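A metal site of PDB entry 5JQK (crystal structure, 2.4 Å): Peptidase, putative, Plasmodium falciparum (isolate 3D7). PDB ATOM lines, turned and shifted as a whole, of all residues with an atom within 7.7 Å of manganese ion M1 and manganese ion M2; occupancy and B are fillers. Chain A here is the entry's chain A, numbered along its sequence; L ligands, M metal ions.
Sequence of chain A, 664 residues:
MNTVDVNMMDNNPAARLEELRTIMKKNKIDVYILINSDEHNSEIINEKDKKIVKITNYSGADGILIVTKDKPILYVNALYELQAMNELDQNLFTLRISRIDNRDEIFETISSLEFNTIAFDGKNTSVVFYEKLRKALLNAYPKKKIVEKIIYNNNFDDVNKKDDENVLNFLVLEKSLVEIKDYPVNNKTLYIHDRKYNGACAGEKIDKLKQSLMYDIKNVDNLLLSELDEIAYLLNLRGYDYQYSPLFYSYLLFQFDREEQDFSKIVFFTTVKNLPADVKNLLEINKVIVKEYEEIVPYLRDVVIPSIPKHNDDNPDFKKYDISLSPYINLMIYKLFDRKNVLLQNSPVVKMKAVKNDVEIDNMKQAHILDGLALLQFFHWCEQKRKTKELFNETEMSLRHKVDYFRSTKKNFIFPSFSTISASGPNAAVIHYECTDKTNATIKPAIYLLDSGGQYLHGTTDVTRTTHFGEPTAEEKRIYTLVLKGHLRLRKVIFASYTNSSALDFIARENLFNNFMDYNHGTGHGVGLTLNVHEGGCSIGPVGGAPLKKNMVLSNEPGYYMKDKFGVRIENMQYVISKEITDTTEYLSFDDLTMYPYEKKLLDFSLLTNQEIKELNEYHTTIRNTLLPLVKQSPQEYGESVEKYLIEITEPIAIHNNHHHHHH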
ATOM      1  N   SER A 417       3.801  -6.286   3.551  1.00  0.00           N
ATOM      2  CA  SER A 417       2.627  -6.658   4.321  1.00  0.00           C
ATOM      3  C   SER A 417       2.252  -8.127   4.128  1.00  0.00           C
ATOM      4  O   SER A 417       1.433  -8.673   4.868  1.00  0.00           O
ATOM      5  CB  SER A 417       1.442  -5.763   3.940  1.00  0.00           C
ATOM      6  OG  SER A 417       1.183  -5.825   2.554  1.00  0.00           O
ATOM      7  N   PHE A 418       2.857  -8.758   3.120  1.00  0.00           N
ATOM      8  CA  PHE A 418       2.739 -10.203   2.925  1.00  0.00           C
ATOM      9  C   PHE A 418       3.797 -10.656   1.933  1.00  0.00           C
ATOM     10  O   PHE A 418       4.514  -9.826   1.369  1.00  0.00           O
ATOM     11  CB  PHE A 418       1.341 -10.605   2.444  1.00  0.00           C
ATOM     12  CG  PHE A 418       0.897  -9.891   1.201  1.00  0.00           C
ATOM     13  CD1 PHE A 418       1.059 -10.477  -0.046  1.00  0.00           C
ATOM     14  CD2 PHE A 418       0.301  -8.646   1.266  1.00  0.00           C
ATOM     15  CE1 PHE A 418       0.641  -9.830  -1.189  1.00  0.00           C
ATOM     16  CE2 PHE A 418      -0.115  -7.987   0.129  1.00  0.00           C
ATOM     17  CZ  PHE A 418       0.048  -8.584  -1.111  1.00  0.00           C
ATOM     18  N   ILE A 421       3.574 -11.967  -4.386  1.00  0.00           N
ATOM     19  CA  ILE A 421       3.309 -12.960  -5.408  1.00  0.00           C
ATOM     20  C   ILE A 421       3.775 -12.419  -6.751  1.00  0.00           C
ATOM     21  O   ILE A 421       3.225 -11.448  -7.280  1.00  0.00           O
ATOM     22  CB  ILE A 421       1.828 -13.333  -5.496  1.00  0.00           C
ATOM     23  CG1 ILE A 421       1.331 -13.837  -4.139  1.00  0.00           C
ATOM     24  CG2 ILE A 421       1.604 -14.378  -6.568  1.00  0.00           C
ATOM     25  CD1 ILE A 421      -0.162 -14.058  -4.095  1.00  0.00           C
ATOM     26  N   LEU A 450       1.457  -9.452 -10.439  1.00  0.00           N
ATOM     27  CA  LEU A 450       2.176  -9.020  -9.242  1.00  0.00           C
ATOM     28  C   LEU A 450       1.206  -8.624  -8.137  1.00  0.00           C
ATOM     29  O   LEU A 450       0.536  -7.590  -8.237  1.00  0.00           O
ATOM     30  CB  LEU A 450       3.104  -7.845  -9.576  1.00  0.00           C
ATOM     31  CG  LEU A 450       3.932  -7.288  -8.423  1.00  0.00           C
ATOM     32  CD1 LEU A 450       5.081  -8.219  -8.088  1.00  0.00           C
ATOM     33  CD2 LEU A 450       4.446  -5.886  -8.723  1.00  0.00           C
ATOM     34  N   ASP A 451       1.168  -9.411  -7.072  1.00  0.00           N
ATOM     35  CA  ASP A 451       0.367  -9.074  -5.890  1.00  0.00           C
ATOM     36  C   ASP A 451       1.335  -8.742  -4.766  1.00  0.00           C
ATOM     37  O   ASP A 451       2.122  -9.578  -4.336  1.00  0.00           O
ATOM     38  CB  ASP A 451      -0.560 -10.220  -5.485  1.00  0.00           C
ATOM     39  CG  ASP A 451      -1.629  -9.783  -4.489  1.00  0.00           C
ATOM     40  OD1 ASP A 451      -1.528  -8.671  -3.938  1.00  0.00           O
ATOM     41  OD2 ASP A 451      -2.585 -10.555  -4.248  1.00  0.00           O
ATOM     42  N   SER A 452       1.277  -7.495  -4.307  1.00  0.00           N
ATOM     43  CA  SER A 452       2.215  -7.023  -3.301  1.00  0.00           C
ATOM     44  C   SER A 452       1.624  -5.905  -2.475  1.00  0.00           C
ATOM     45  O   SER A 452       0.598  -5.309  -2.834  1.00  0.00           O
ATOM     46  CB  SER A 452       3.509  -6.556  -3.954  1.00  0.00           C
ATOM     47  OG  SER A 452       3.265  -5.475  -4.849  1.00  0.00           O
ATOM     48  N   GLY A 453       2.255  -5.637  -1.339  1.00  0.00           N
ATOM     49  CA  GLY A 453       1.832  -4.572  -0.466  1.00  0.00           C
ATOM     50  C   GLY A 453       2.911  -4.326   0.562  1.00  0.00           C
ATOM     51  O   GLY A 453       3.920  -5.037   0.604  1.00  0.00           O
ATOM     52  N   THR A 461      -1.026  -1.713   2.869  1.00  0.00           N
ATOM     53  CA  THR A 461      -1.441  -1.696   1.475  1.00  0.00           C
ATOM     54  C   THR A 461      -1.470  -3.082   0.865  1.00  0.00           C
ATOM     55  O   THR A 461      -0.681  -3.951   1.215  1.00  0.00           O
ATOM     56  CB  THR A 461      -0.504  -0.824   0.631  1.00  0.00           C
ATOM     57  OG1 THR A 461       0.792  -1.419   0.583  1.00  0.00           O
ATOM     58  CG2 THR A 461      -0.396   0.577   1.220  1.00  0.00           C
ATOM     59  N   ASP A 462      -2.427  -3.293  -0.037  1.00  0.00           N
ATOM     60  CA  ASP A 462      -2.542  -4.533  -0.795  1.00  0.00           C
ATOM     61  C   ASP A 462      -2.972  -4.196  -2.229  1.00  0.00           C
ATOM     62  O   ASP A 462      -4.030  -3.615  -2.432  1.00  0.00           O
ATOM     63  CB  ASP A 462      -3.544  -5.473  -0.106  1.00  0.00           C
ATOM     64  CG  ASP A 462      -3.653  -6.830  -0.770  1.00  0.00           C
ATOM     65  OD1 ASP A 462      -4.512  -7.610  -0.341  1.00  0.00           O
ATOM     66  OD2 ASP A 462      -2.894  -7.120  -1.724  1.00  0.00           O
ATOM     67  N   VAL A 463      -2.157  -4.557  -3.215  1.00  0.00           N
ATOM     68  CA  VAL A 463      -2.472  -4.211  -4.598  1.00  0.00           C
ATOM     69  C   VAL A 463      -2.001  -5.276  -5.587  1.00  0.00           C
ATOM     70  O   VAL A 463      -0.910  -5.819  -5.439  1.00  0.00           O
ATOM     71  CB  VAL A 463      -1.837  -2.838  -4.987  1.00  0.00           C
ATOM     72  CG1 VAL A 463      -0.367  -2.776  -4.590  1.00  0.00           C
ATOM     73  CG2 VAL A 463      -2.013  -2.538  -6.476  1.00  0.00           C
ATOM     74  N   THR A 464      -2.834  -5.569  -6.581  1.00  0.00           N
ATOM     75  CA  THR A 464      -2.432  -6.472  -7.657  1.00  0.00           C
ATOM     76  C   THR A 464      -2.583  -5.799  -9.010  1.00  0.00           C
ATOM     77  O   THR A 464      -3.603  -5.166  -9.300  1.00  0.00           O
ATOM     78  CB  THR A 464      -3.255  -7.779  -7.671  1.00  0.00           C
ATOM     79  OG1 THR A 464      -3.311  -8.334  -6.360  1.00  0.00           O
ATOM     80  CG2 THR A 464      -2.648  -8.783  -8.640  1.00  0.00           C
ATOM     81  N   ARG A 465      -1.560  -5.944  -9.845  1.00  0.00           N
ATOM     82  CA  ARG A 465      -1.647  -5.518 -11.227  1.00  0.00           C
ATOM     83  C   ARG A 465      -1.201  -6.655 -12.124  1.00  0.00           C
ATOM     84  O   ARG A 465      -0.298  -7.404 -11.774  1.00  0.00           O
ATOM     85  CB  ARG A 465      -0.810  -4.261 -11.477  1.00  0.00           C
ATOM     86  CG  ARG A 465      -1.398  -2.995 -10.896  1.00  0.00           C
ATOM     87  CD  ARG A 465      -2.781  -2.752 -11.475  1.00  0.00           C
ATOM     88  NE  ARG A 465      -3.360  -1.479 -11.044  1.00  0.00           N
ATOM     89  CZ  ARG A 465      -4.228  -1.351 -10.050  1.00  0.00           C
ATOM     90  NH1 ARG A 465      -4.616  -2.411  -9.359  1.00  0.00           N
ATOM     91  NH2 ARG A 465      -4.714  -0.158  -9.740  1.00  0.00           N
ATOM     92  N   GLY A 522     -12.455 -14.991  -2.667  1.00  0.00           N
ATOM     93  CA  GLY A 522     -13.386 -13.911  -2.394  1.00  0.00           C
ATOM     94  C   GLY A 522     -13.019 -12.684  -3.216  1.00  0.00           C
ATOM     95  O   GLY A 522     -11.922 -12.595  -3.749  1.00  0.00           O
ATOM     96  N   THR A 523     -13.965 -11.753  -3.340  1.00  0.00           N
ATOM     97  CA  THR A 523     -13.717 -10.561  -4.135  1.00  0.00           C
ATOM     98  C   THR A 523     -12.943  -9.512  -3.338  1.00  0.00           C
ATOM     99  O   THR A 523     -12.111  -8.794  -3.895  1.00  0.00           O
ATOM    100  CB  THR A 523     -15.026  -9.945  -4.641  1.00  0.00           C
ATOM    101  OG1 THR A 523     -15.709 -10.901  -5.461  1.00  0.00           O
ATOM    102  CG2 THR A 523     -14.739  -8.702  -5.472  1.00  0.00           C
ATOM    103  N   GLY A 524     -13.196  -9.444  -2.039  1.00  0.00           N
ATOM    104  CA  GLY A 524     -12.484  -8.491  -1.204  1.00  0.00           C
ATOM    105  C   GLY A 524     -12.428  -8.851   0.262  1.00  0.00           C
ATOM    106  O   GLY A 524     -13.314  -9.526   0.794  1.00  0.00           O
ATOM    107  N   HIS A 525     -11.384  -8.376   0.918  1.00  0.00           N
ATOM    108  CA  HIS A 525     -11.187  -8.594   2.346  1.00  0.00           C
ATOM    109  C   HIS A 525     -10.974  -7.255   3.021  1.00  0.00           C
ATOM    110  O   HIS A 525     -10.534  -6.294   2.374  1.00  0.00           O
ATOM    111  CB  HIS A 525      -9.982  -9.510   2.599  1.00  0.00           C
ATOM    112  CG  HIS A 525      -8.724  -9.043   1.941  1.00  0.00           C
ATOM    113  ND1 HIS A 525      -7.962  -8.009   2.442  1.00  0.00           N
ATOM    114  CD2 HIS A 525      -8.087  -9.476   0.823  1.00  0.00           C
ATOM    115  CE1 HIS A 525      -6.917  -7.810   1.659  1.00  0.00           C
ATOM    116  NE2 HIS A 525      -6.972  -8.693   0.664  1.00  0.00           N
ATOM    117  N   GLY A 526     -11.272  -7.184   4.309  1.00  0.00           N
ATOM    118  CA  GLY A 526     -10.977  -5.979   5.074  1.00  0.00           C
ATOM    119  C   GLY A 526      -9.479  -5.870   5.234  1.00  0.00           C
ATOM    120  O   GLY A 526      -8.770  -6.860   5.116  1.00  0.00           O
ATOM    121  N   VAL A 527      -8.992  -4.651   5.473  1.00  0.00           N
ATOM    122  CA  VAL A 527      -7.558  -4.431   5.664  1.00  0.00           C
ATOM    123  C   VAL A 527      -7.306  -3.565   6.888  1.00  0.00           C
ATOM    124  O   VAL A 527      -7.903  -2.506   7.045  1.00  0.00           O
ATOM    125  CB  VAL A 527      -6.914  -3.775   4.428  1.00  0.00           C
ATOM    126  CG1 VAL A 527      -5.414  -3.607   4.641  1.00  0.00           C
ATOM    127  CG2 VAL A 527      -7.177  -4.615   3.183  1.00  0.00           C
ATOM    128  N   VAL A 533      -2.901  -7.579   6.713  1.00  0.00           N
ATOM    129  CA  VAL A 533      -3.367  -7.306   5.374  1.00  0.00           C
ATOM    130  C   VAL A 533      -4.722  -7.980   5.156  1.00  0.00           C
ATOM    131  O   VAL A 533      -5.506  -7.569   4.307  1.00  0.00           O
ATOM    132  CB  VAL A 533      -2.328  -7.770   4.329  1.00  0.00           C
ATOM    133  CG1 VAL A 533      -2.231  -9.285   4.302  1.00  0.00           C
ATOM    134  CG2 VAL A 533      -2.658  -7.215   2.957  1.00  0.00           C
ATOM    135  N   HIS A 534      -5.008  -9.026   5.937  1.00  0.00           N
ATOM    136  CA  HIS A 534      -6.337  -9.636   5.957  1.00  0.00           C
ATOM    137  C   HIS A 534      -7.006  -9.410   7.302  1.00  0.00           C
ATOM    138  O   HIS A 534      -6.636 -10.009   8.307  1.00  0.00           O
ATOM    139  CB  HIS A 534      -6.248 -11.135   5.668  1.00  0.00           C
ATOM    140  CG  HIS A 534      -5.748 -11.450   4.292  1.00  0.00           C
ATOM    141  ND1 HIS A 534      -5.094 -12.621   3.988  1.00  0.00           N
ATOM    142  CD2 HIS A 534      -5.812 -10.740   3.134  1.00  0.00           C
ATOM    143  CE1 HIS A 534      -4.766 -12.626   2.703  1.00  0.00           C
ATOM    144  NE2 HIS A 534      -5.191 -11.495   2.166  1.00  0.00           N
ATOM    145  N   LEU A 554     -11.779  -1.891   2.213  1.00  0.00           N
ATOM    146  CA  LEU A 554     -11.842  -3.203   1.607  1.00  0.00           C
ATOM    147  C   LEU A 554     -11.010  -3.312   0.337  1.00  0.00           C
ATOM    148  O   LEU A 554     -10.776  -2.306  -0.348  1.00  0.00           O
ATOM    149  CB  LEU A 554     -13.306  -3.570   1.288  1.00  0.00           C
ATOM    150  CG  LEU A 554     -14.205  -3.722   2.513  1.00  0.00           C
ATOM    151  CD1 LEU A 554     -15.485  -2.933   2.346  1.00  0.00           C
ATOM    152  CD2 LEU A 554     -14.496  -5.185   2.781  1.00  0.00           C
ATOM    153  N   SER A 555     -10.551  -4.508   0.041  1.00  0.00           N
ATOM    154  CA  SER A 555      -9.937  -4.780  -1.243  1.00  0.00           C
ATOM    155  C   SER A 555     -11.002  -5.019  -2.304  1.00  0.00           C
ATOM    156  O   SER A 555     -12.128  -5.400  -1.993  1.00  0.00           O
ATOM    157  CB  SER A 555      -8.977  -5.975  -1.149  1.00  0.00           C
ATOM    158  OG  SER A 555      -9.677  -7.183  -0.923  1.00  0.00           O
ATOM    159  N   ASN A 556     -10.651  -4.760  -3.555  1.00  0.00           N
ATOM    160  CA  ASN A 556     -11.498  -5.110  -4.673  1.00  0.00           C
ATOM    161  C   ASN A 556     -10.613  -5.876  -5.658  1.00  0.00           C
ATOM    162  O   ASN A 556      -9.819  -5.266  -6.359  1.00  0.00           O
ATOM    163  CB  ASN A 556     -12.091  -3.834  -5.285  1.00  0.00           C
ATOM    164  CG  ASN A 556     -12.675  -4.024  -6.680  1.00  0.00           C
ATOM    165  OD1 ASN A 556     -12.952  -5.140  -7.127  1.00  0.00           O
ATOM    166  ND2 ASN A 556     -12.850  -2.917  -7.382  1.00  0.00           N
ATOM    167  N   GLU A 557     -10.779  -7.188  -5.739  1.00  0.00           N
ATOM    168  CA  GLU A 557      -9.838  -8.000  -6.508  1.00  0.00           C
ATOM    169  C   GLU A 557     -10.429  -9.201  -7.219  1.00  0.00           C
ATOM    170  O   GLU A 557     -10.115 -10.342  -6.880  1.00  0.00           O
ATOM    171  CB  GLU A 557      -8.683  -8.491  -5.611  1.00  0.00           C
ATOM    172  CG  GLU A 557      -9.071  -9.029  -4.245  1.00  0.00           C
ATOM    173  CD  GLU A 557      -7.854  -9.434  -3.429  1.00  0.00           C
ATOM    174  OE1 GLU A 557      -6.872  -9.924  -4.025  1.00  0.00           O
ATOM    175  OE2 GLU A 557      -7.864  -9.261  -2.186  1.00  0.00           O
ATOM    176  N   ARG A 569      -5.366 -11.107 -12.142  1.00  0.00           N
ATOM    177  CA  ARG A 569      -6.061 -10.486 -11.021  1.00  0.00           C
ATOM    178  C   ARG A 569      -5.820  -8.986 -11.023  1.00  0.00           C
ATOM    179  O   ARG A 569      -4.704  -8.530 -11.307  1.00  0.00           O
ATOM    180  CB  ARG A 569      -5.644 -11.095  -9.676  1.00  0.00           C
ATOM    181  CG  ARG A 569      -6.368 -10.499  -8.481  1.00  0.00           C
ATOM    182  CD  ARG A 569      -6.241 -11.349  -7.213  1.00  0.00           C
ATOM    183  NE  ARG A 569      -4.863 -11.450  -6.729  1.00  0.00           N
ATOM    184  CZ  ARG A 569      -4.099 -12.524  -6.886  1.00  0.00           C
ATOM    185  NH1 ARG A 569      -4.574 -13.588  -7.518  1.00  0.00           N
ATOM    186  NH2 ARG A 569      -2.860 -12.534  -6.409  1.00  0.00           N
ATOM    187  N   GLU A 571      -6.409  -5.754  -8.494  1.00  0.00           N
ATOM    188  CA  GLU A 571      -6.770  -5.445  -7.110  1.00  0.00           C
ATOM    189  C   GLU A 571      -6.535  -4.000  -6.697  1.00  0.00           C
ATOM    190  O   GLU A 571      -5.447  -3.452  -6.884  1.00  0.00           O
ATOM    191  CB  GLU A 571      -6.013  -6.365  -6.148  1.00  0.00           C
ATOM    192  CG  GLU A 571      -6.259  -6.060  -4.669  1.00  0.00           C
ATOM    193  CD  GLU A 571      -5.506  -7.000  -3.748  1.00  0.00           C
ATOM    194  OE1 GLU A 571      -4.485  -7.572  -4.165  1.00  0.00           O
ATOM    195  OE2 GLU A 571      -5.954  -7.168  -2.595  1.00  0.00           O
ATOM    196  N   ASN A 572      -7.568  -3.399  -6.139  1.00  0.00           N
ATOM    197  CA  ASN A 572      -7.471  -2.101  -5.497  1.00  0.00           C
ATOM    198  C   ASN A 572      -7.911  -2.200  -4.043  1.00  0.00           C
ATOM    199  O   ASN A 572      -8.580  -3.157  -3.659  1.00  0.00           O
ATOM    200  CB  ASN A 572      -8.327  -1.062  -6.200  1.00  0.00           C
ATOM    201  CG  ASN A 572      -7.643  -0.448  -7.392  1.00  0.00           C
ATOM    202  OD1 ASN A 572      -6.647  -0.972  -7.887  1.00  0.00           O
ATOM    203  ND2 ASN A 572      -8.176   0.674  -7.863  1.00  0.00           N
ATOM    204  N   MET A 573      -7.513  -1.229  -3.245  1.00  0.00           N
ATOM    205  CA  MET A 573      -8.147  -1.026  -1.944  1.00  0.00           C
ATOM    206  C   MET A 573      -9.001   0.231  -2.048  1.00  0.00           C
ATOM    207  O   MET A 573      -8.648   1.176  -2.752  1.00  0.00           O
ATOM    208  CB  MET A 573      -7.122  -0.919  -0.827  1.00  0.00           C
ATOM    209  CG  MET A 573      -6.673  -2.251  -0.239  1.00  0.00           C
ATOM    210  SD  MET A 573      -5.196  -2.055   0.784  1.00  0.00           S
ATOM    211  CE  MET A 573      -5.881  -1.124   2.144  1.00  0.00           C
HETATM  212  P1  LIG L   1      -3.898 -11.058  -0.952  1.00  0.00           P
HETATM  213  O1  LIG L   1      -2.969 -10.450   0.084  1.00  0.00           O
HETATM  214  O2  LIG L   1      -4.418  -9.982  -1.877  1.00  0.00           O
HETATM  215  O3  LIG L   1      -5.059 -11.718  -0.262  1.00  0.00           O
HETATM  216  O4  LIG L   1      -3.134 -12.092  -1.755  1.00  0.00           O
HETATM  217 MN    MN M   1      -5.898  -8.659  -1.221  1.00  0.00          MN
HETATM  218 MN    MN M   2      -3.193  -8.618  -2.887  1.00  0.00          MN
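Within 4 Å of manganese ion M1: Asp 462, His 525, Glu 557 and Glu 571.
The nearest printed residue that does not touch manganese ion M1 is Ser 555 (4.1 Å).
SD of Met 573 lies within hydrogen-bond range of N of Asp 462 (3.1 Å).
The side-chain hydroxyl (OG1) of Thr 464 lies close to the side-chain carboxylate (OD1) of Asp 451 (3.0 Å).
The side-chain carboxylate (OD2) of Asp 451 sits close to the guanidinium group (NH2) of Arg 569.
N of Ile 421 lies within hydrogen-bond range of O of Asp 451 (2.8 Å).
The backbone carbonyl oxygen (O) of Glu 571 is in hydrogen-bond range of the guanidinium group (NH1) of Arg 465, at 2.8 Å.
The backbone NH of His 525 lies within hydrogen-bond range of the side-chain hydroxyl of Ser 555 (2.8 Å).
OE2 of Glu 557 lies close to OG of Ser 555 (3.0 Å).
NE of Arg 569 is in salt-bridge range of OE1 of Glu 557 (3.7 Å).
The side-chain carboxylate (OD2) of Asp 462 binds manganese ion M2, at 1.9 Å.
Manganese ion M2 is bound by OD1 of Asp 451.
Manganese ion M2 is bound by O2 of the ligand (2.1 Å).
Manganese ion M2 is bound by OE1 of Glu 571, at 2.1 Å.
OD2 of Asp 451 binds manganese ion M2, 2.4 Å away.
Manganese ion M1 is bound by OD1 of Asp 462 (1.9 Å), OE2 of Glu 571 (2.0 Å), O2 of the ligand (2.1 Å), NE2 of His 525 (2.2 Å) and OE2 of Glu 557 (2.3 Å).
Manganese ion M1 has five donor atoms within binding distance.
Residues that only touch manganese ion M2: Phe 418 and Thr 464.
Within 4 Å of manganese ion M2: Phe 418, Asp 451, Asp 462, Thr 464 and Glu 571.
The nearest printed residue that does not touch manganese ion M2 is Glu 557 (4.1 Å).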
